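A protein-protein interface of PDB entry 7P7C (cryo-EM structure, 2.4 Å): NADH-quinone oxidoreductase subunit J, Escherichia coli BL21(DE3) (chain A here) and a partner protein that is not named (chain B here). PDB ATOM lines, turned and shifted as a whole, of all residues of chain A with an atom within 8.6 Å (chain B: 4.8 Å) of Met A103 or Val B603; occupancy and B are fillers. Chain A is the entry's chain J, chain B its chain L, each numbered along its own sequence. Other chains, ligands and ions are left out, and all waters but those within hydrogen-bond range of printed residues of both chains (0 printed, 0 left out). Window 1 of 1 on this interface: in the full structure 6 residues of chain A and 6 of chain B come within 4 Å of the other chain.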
ATOM      1  N   PRO A  96      40.690  20.394  -3.633  1.00  0.00           N
ATOM      2  CA  PRO A  96      39.936  19.151  -3.873  1.00  0.00           C
ATOM      3  C   PRO A  96      39.053  18.715  -2.715  1.00  0.00           C
ATOM      4  O   PRO A  96      37.983  18.145  -2.959  1.00  0.00           O
ATOM      5  CB  PRO A  96      41.044  18.129  -4.145  1.00  0.00           C
ATOM      6  CG  PRO A  96      42.135  18.933  -4.747  1.00  0.00           C
ATOM      7  CD  PRO A  96      42.089  20.277  -4.093  1.00  0.00           C
ATOM      8  N   ALA A  97      39.456  18.978  -1.470  1.00  0.00           N
ATOM      9  CA  ALA A  97      38.635  18.589  -0.327  1.00  0.00           C
ATOM     10  C   ALA A  97      37.317  19.351  -0.303  1.00  0.00           C
ATOM     11  O   ALA A  97      36.250  18.752  -0.132  1.00  0.00           O
ATOM     12  CB  ALA A  97      39.400  18.803   0.976  1.00  0.00           C
ATOM     13  N   ILE A  98      37.361  20.673  -0.495  1.00  0.00           N
ATOM     14  CA  ILE A  98      36.112  21.429  -0.467  1.00  0.00           C
ATOM     15  C   ILE A  98      35.303  21.170  -1.732  1.00  0.00           C
ATOM     16  O   ILE A  98      34.069  21.227  -1.702  1.00  0.00           O
ATOM     17  CB  ILE A  98      36.357  22.938  -0.250  1.00  0.00           C
ATOM     18  CG1 ILE A  98      37.215  23.542  -1.361  1.00  0.00           C
ATOM     19  CG2 ILE A  98      36.987  23.176   1.118  1.00  0.00           C
ATOM     20  CD1 ILE A  98      37.713  24.944  -1.070  1.00  0.00           C
ATOM     21  N   LEU A  99      35.969  20.860  -2.850  1.00  0.00           N
ATOM     22  CA  LEU A  99      35.250  20.486  -4.066  1.00  0.00           C
ATOM     23  C   LEU A  99      34.455  19.199  -3.863  1.00  0.00           C
ATOM     24  O   LEU A  99      33.265  19.118  -4.209  1.00  0.00           O
ATOM     25  CB  LEU A  99      36.244  20.334  -5.215  1.00  0.00           C
ATOM     26  CG  LEU A  99      35.677  20.202  -6.622  1.00  0.00           C
ATOM     27  CD1 LEU A  99      35.094  21.528  -7.073  1.00  0.00           C
ATOM     28  CD2 LEU A  99      36.763  19.737  -7.566  1.00  0.00           C
ATOM     29  N   SER A 100      35.095  18.188  -3.269  1.00  0.00           N
ATOM     30  CA  SER A 100      34.406  16.943  -2.957  1.00  0.00           C
ATOM     31  C   SER A 100      33.336  17.143  -1.897  1.00  0.00           C
ATOM     32  O   SER A 100      32.300  16.476  -1.941  1.00  0.00           O
ATOM     33  CB  SER A 100      35.413  15.890  -2.503  1.00  0.00           C
ATOM     34  OG  SER A 100      36.371  15.638  -3.515  1.00  0.00           O
ATOM     35  N   ALA A 101      33.557  18.059  -0.951  1.00  0.00           N
ATOM     36  CA  ALA A 101      32.542  18.352   0.055  1.00  0.00           C
ATOM     37  C   ALA A 101      31.310  19.004  -0.564  1.00  0.00           C
ATOM     38  O   ALA A 101      30.179  18.700  -0.170  1.00  0.00           O
ATOM     39  CB  ALA A 101      33.131  19.244   1.145  1.00  0.00           C
ATOM     40  N   ILE A 102      31.511  19.905  -1.530  1.00  0.00           N
ATOM     41  CA  ILE A 102      30.390  20.530  -2.228  1.00  0.00           C
ATOM     42  C   ILE A 102      29.618  19.495  -3.038  1.00  0.00           C
ATOM     43  O   ILE A 102      28.377  19.463  -3.014  1.00  0.00           O
ATOM     44  CB  ILE A 102      30.897  21.687  -3.107  1.00  0.00           C
ATOM     45  CG1 ILE A 102      31.332  22.867  -2.238  1.00  0.00           C
ATOM     46  CG2 ILE A 102      29.830  22.137  -4.090  1.00  0.00           C
ATOM     47  CD1 ILE A 102      32.153  23.892  -2.978  1.00  0.00           C
ATOM     48  N   MET A 103      30.337  18.623  -3.755  1.00  0.00           N
ATOM     49  CA  MET A 103      29.670  17.558  -4.503  1.00  0.00           C
ATOM     50  C   MET A 103      28.895  16.629  -3.572  1.00  0.00           C
ATOM     51  O   MET A 103      27.753  16.248  -3.868  1.00  0.00           O
ATOM     52  CB  MET A 103      30.695  16.775  -5.322  1.00  0.00           C
ATOM     53  CG  MET A 103      30.086  15.736  -6.244  1.00  0.00           C
ATOM     54  SD  MET A 103      31.336  14.776  -7.110  1.00  0.00           S
ATOM     55  CE  MET A 103      32.209  16.082  -7.960  1.00  0.00           C
ATOM     56  N   LEU A 104      29.485  16.295  -2.422  1.00  0.00           N
ATOM     57  CA  LEU A 104      28.828  15.436  -1.449  1.00  0.00           C
ATOM     58  C   LEU A 104      27.579  16.087  -0.872  1.00  0.00           C
ATOM     59  O   LEU A 104      26.561  15.415  -0.692  1.00  0.00           O
ATOM     60  CB  LEU A 104      29.807  15.073  -0.332  1.00  0.00           C
ATOM     61  CG  LEU A 104      29.241  14.380   0.909  1.00  0.00           C
ATOM     62  CD1 LEU A 104      28.685  13.013   0.558  1.00  0.00           C
ATOM     63  CD2 LEU A 104      30.303  14.267   1.986  1.00  0.00           C
ATOM     64  N   VAL A 105      27.629  17.389  -0.575  1.00  0.00           N
ATOM     65  CA  VAL A 105      26.455  18.015   0.025  1.00  0.00           C
ATOM     66  C   VAL A 105      25.335  18.161  -1.003  1.00  0.00           C
ATOM     67  O   VAL A 105      24.155  18.034  -0.654  1.00  0.00           O
ATOM     68  CB  VAL A 105      26.812  19.351   0.718  1.00  0.00           C
ATOM     69  CG1 VAL A 105      27.104  20.470  -0.264  1.00  0.00           C
ATOM     70  CG2 VAL A 105      25.707  19.759   1.683  1.00  0.00           C
ATOM     71  N   VAL A 106      25.670  18.362  -2.285  1.00  0.00           N
ATOM     72  CA  VAL A 106      24.629  18.386  -3.312  1.00  0.00           C
ATOM     73  C   VAL A 106      23.986  17.007  -3.469  1.00  0.00           C
ATOM     74  O   VAL A 106      22.752  16.884  -3.539  1.00  0.00           O
ATOM     75  CB  VAL A 106      25.198  18.909  -4.644  1.00  0.00           C
ATOM     76  CG1 VAL A 106      24.167  18.787  -5.747  1.00  0.00           C
ATOM     77  CG2 VAL A 106      25.623  20.356  -4.501  1.00  0.00           C
ATOM     78  N   ILE A 107      24.807  15.948  -3.495  1.00  0.00           N
ATOM     79  CA  ILE A 107      24.276  14.588  -3.613  1.00  0.00           C
ATOM     80  C   ILE A 107      23.425  14.231  -2.397  1.00  0.00           C
ATOM     81  O   ILE A 107      22.363  13.609  -2.525  1.00  0.00           O
ATOM     82  CB  ILE A 107      25.425  13.583  -3.826  1.00  0.00           C
ATOM     83  CG1 ILE A 107      26.079  13.801  -5.188  1.00  0.00           C
ATOM     84  CG2 ILE A 107      24.932  12.156  -3.745  1.00  0.00           C
ATOM     85  CD1 ILE A 107      27.471  13.224  -5.295  1.00  0.00           C
ATOM     86  N   VAL A 108      23.862  14.640  -1.204  1.00  0.00           N
ATOM     87  CA  VAL A 108      23.119  14.341   0.016  1.00  0.00           C
ATOM     88  C   VAL A 108      21.797  15.102   0.042  1.00  0.00           C
ATOM     89  O   VAL A 108      20.770  14.562   0.469  1.00  0.00           O
ATOM     90  CB  VAL A 108      23.997  14.638   1.249  1.00  0.00           C
ATOM     91  CG1 VAL A 108      23.165  14.802   2.510  1.00  0.00           C
ATOM     92  CG2 VAL A 108      25.003  13.520   1.444  1.00  0.00           C
ATOM     93  N   TYR A 109      21.790  16.349  -0.450  1.00  0.00           N
ATOM     94  CA  TYR A 109      20.538  17.093  -0.569  1.00  0.00           C
ATOM     95  C   TYR A 109      19.576  16.389  -1.517  1.00  0.00           C
ATOM     96  O   TYR A 109      18.367  16.339  -1.260  1.00  0.00           O
ATOM     97  CB  TYR A 109      20.836  18.544  -0.998  1.00  0.00           C
ATOM     98  CG  TYR A 109      19.708  19.383  -1.618  1.00  0.00           C
ATOM     99  CD1 TYR A 109      19.256  19.185  -2.929  1.00  0.00           C
ATOM    100  CD2 TYR A 109      19.076  20.365  -0.864  1.00  0.00           C
ATOM    101  CE1 TYR A 109      18.231  19.943  -3.459  1.00  0.00           C
ATOM    102  CE2 TYR A 109      18.050  21.128  -1.391  1.00  0.00           C
ATOM    103  CZ  TYR A 109      17.633  20.913  -2.686  1.00  0.00           C
ATOM    104  OH  TYR A 109      16.613  21.670  -3.211  1.00  0.00           O
ATOM    105  N   ALA A 110      20.092  15.855  -2.626  1.00  0.00           N
ATOM    106  CA  ALA A 110      19.238  15.106  -3.546  1.00  0.00           C
ATOM    107  C   ALA A 110      18.698  13.832  -2.902  1.00  0.00           C
ATOM    108  O   ALA A 110      17.541  13.461  -3.123  1.00  0.00           O
ATOM    109  CB  ALA A 110      20.004  14.778  -4.821  1.00  0.00           C
ATOM    110  N   ILE A 111      19.528  13.149  -2.112  1.00  0.00           N
ATOM    111  CA  ILE A 111      19.114  11.912  -1.453  1.00  0.00           C
ATOM    112  C   ILE A 111      18.054  12.189  -0.389  1.00  0.00           C
ATOM    113  O   ILE A 111      17.106  11.411  -0.217  1.00  0.00           O
ATOM    114  CB  ILE A 111      20.352  11.200  -0.869  1.00  0.00           C
ATOM    115  CG1 ILE A 111      21.164  10.546  -1.986  1.00  0.00           C
ATOM    116  CG2 ILE A 111      19.979  10.151   0.163  1.00  0.00           C
ATOM    117  CD1 ILE A 111      22.583  10.237  -1.594  1.00  0.00           C
ATOM    118  N   SER B 599      35.641  16.785 -12.052  1.00  0.00           N
ATOM    119  CA  SER B 599      34.889  16.921 -10.804  1.00  0.00           C
ATOM    120  C   SER B 599      34.259  18.307 -10.670  1.00  0.00           C
ATOM    121  O   SER B 599      33.148  18.440 -10.140  1.00  0.00           O
ATOM    122  CB  SER B 599      35.789  16.615  -9.607  1.00  0.00           C
ATOM    123  OG  SER B 599      37.036  17.266  -9.721  1.00  0.00           O
ATOM    124  N   ILE B 600      34.947  19.348 -11.154  1.00  0.00           N
ATOM    125  CA  ILE B 600      34.383  20.700 -11.165  1.00  0.00           C
ATOM    126  C   ILE B 600      33.151  20.757 -12.060  1.00  0.00           C
ATOM    127  O   ILE B 600      32.124  21.341 -11.692  1.00  0.00           O
ATOM    128  CB  ILE B 600      35.451  21.721 -11.606  1.00  0.00           C
ATOM    129  CG1 ILE B 600      36.456  21.977 -10.486  1.00  0.00           C
ATOM    130  CG2 ILE B 600      34.820  23.040 -12.020  1.00  0.00           C
ATOM    131  CD1 ILE B 600      37.747  22.591 -10.966  1.00  0.00           C
ATOM    132  N   GLY B 601      33.233  20.148 -13.245  1.00  0.00           N
ATOM    133  CA  GLY B 601      32.078  20.095 -14.123  1.00  0.00           C
ATOM    134  C   GLY B 601      30.937  19.284 -13.546  1.00  0.00           C
ATOM    135  O   GLY B 601      29.767  19.612 -13.752  1.00  0.00           O
ATOM    136  N   ALA B 602      31.260  18.218 -12.810  1.00  0.00           N
ATOM    137  CA  ALA B 602      30.230  17.466 -12.105  1.00  0.00           C
ATOM    138  C   ALA B 602      29.539  18.328 -11.059  1.00  0.00           C
ATOM    139  O   ALA B 602      28.309  18.293 -10.930  1.00  0.00           O
ATOM    140  CB  ALA B 602      30.835  16.222 -11.459  1.00  0.00           C
ATOM    141  N   VAL B 603      30.320  19.119 -10.316  1.00  0.00           N
ATOM    142  CA  VAL B 603      29.761  20.027  -9.315  1.00  0.00           C
ATOM    143  C   VAL B 603      28.847  21.054  -9.974  1.00  0.00           C
ATOM    144  O   VAL B 603      27.733  21.312  -9.501  1.00  0.00           O
ATOM    145  CB  VAL B 603      30.903  20.698  -8.525  1.00  0.00           C
ATOM    146  CG1 VAL B 603      30.456  22.011  -7.904  1.00  0.00           C
ATOM    147  CG2 VAL B 603      31.428  19.760  -7.457  1.00  0.00           C
ATOM    148  N   VAL B 604      29.296  21.630 -11.093  1.00  0.00           N
ATOM    149  CA  VAL B 604      28.521  22.652 -11.792  1.00  0.00           C
ATOM    150  C   VAL B 604      27.224  22.070 -12.346  1.00  0.00           C
ATOM    151  O   VAL B 604      26.153  22.670 -12.200  1.00  0.00           O
ATOM    152  CB  VAL B 604      29.381  23.295 -12.898  1.00  0.00           C
ATOM    153  CG1 VAL B 604      28.526  24.110 -13.854  1.00  0.00           C
ATOM    154  CG2 VAL B 604      30.462  24.163 -12.281  1.00  0.00           C
ATOM    155  N   VAL B 605      27.297  20.888 -12.965  1.00  0.00           N
ATOM    156  CA  VAL B 605      26.110  20.244 -13.527  1.00  0.00           C
ATOM    157  C   VAL B 605      25.114  19.891 -12.428  1.00  0.00           C
ATOM    158  O   VAL B 605      23.907  20.127 -12.567  1.00  0.00           O
ATOM    159  CB  VAL B 605      26.523  19.008 -14.352  1.00  0.00           C
ATOM    160  CG1 VAL B 605      25.354  18.060 -14.557  1.00  0.00           C
ATOM    161  CG2 VAL B 605      27.092  19.434 -15.691  1.00  0.00           C
ATOM    162  N   LEU B 606      25.605  19.348 -11.309  1.00  0.00           N
ATOM    163  CA  LEU B 606      24.724  18.975 -10.207  1.00  0.00           C
ATOM    164  C   LEU B 606      24.059  20.197  -9.580  1.00  0.00           C
ATOM    165  O   LEU B 606      22.855  20.174  -9.292  1.00  0.00           O
ATOM    166  CB  LEU B 606      25.514  18.195  -9.158  1.00  0.00           C
ATOM    167  CG  LEU B 606      25.431  16.667  -9.177  1.00  0.00           C
ATOM    168  CD1 LEU B 606      25.782  16.099 -10.541  1.00  0.00           C
ATOM    169  CD2 LEU B 606      26.353  16.101  -8.116  1.00  0.00           C
ATOM    170  N   ALA B 607      24.819  21.278  -9.380  1.00  0.00           N
ATOM    171  CA  ALA B 607      24.249  22.502  -8.825  1.00  0.00           C
ATOM    172  C   ALA B 607      23.229  23.126  -9.771  1.00  0.00           C
ATOM    173  O   ALA B 607      22.169  23.589  -9.330  1.00  0.00           O
ATOM    174  CB  ALA B 607      25.362  23.498  -8.502  1.00  0.00           C
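Among the printed residues, merely in contact across the chains: Leu A99 with Ser B599 (3.3 Å), Leu A99 with Ile B600 (3.7 Å), Leu A99 with Val B603 (3.8 Å), Ile A102 with Val B603 (3.9 Å), Met A103 with Ser B599 (3.3 Å), Met A103 with Ala B602 (3.8 Å), Met A103 with Val B603 (3.7 Å), Val A106 with Leu B606 (3.7 Å) and Ile A107 with Leu B606 (3.7 Å).
Printed residues of chain B within 4 Å of Met A103: Ser B599 (3.3 Å), Ala B602 (3.8 Å) and Val B603 (3.7 Å).
Val B603 touches just these residues of chain A: Leu A99 (3.8 Å), Ile A102 (3.9 Å) and Met A103 (3.7 Å).
Of the printed residues of chain A, Ile B600 touches Leu A99 (3.7 Å).
Of the printed residues of chain A, Leu B606 touches Val A106 (3.7 Å) and Ile A107 (3.7 Å).
Of the printed residues of chain A, Ser B599 touches Leu A99 and Met A103.
Printed residues of chain B within 4 Å of Ile A102: Val B603 (3.9 Å).
The nearest residue of chain A that does not touch Val B603 is Val A106 (5.5 Å).
Of the 16 printed residues of chain A, 5 touch a printed residue of chain B.
Hydrophobic or aromatic side chains of chain A within 4 Å of the printed part of chain B: Leu A99, Ile A102, Met A103, Val A106 and Ile A107.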
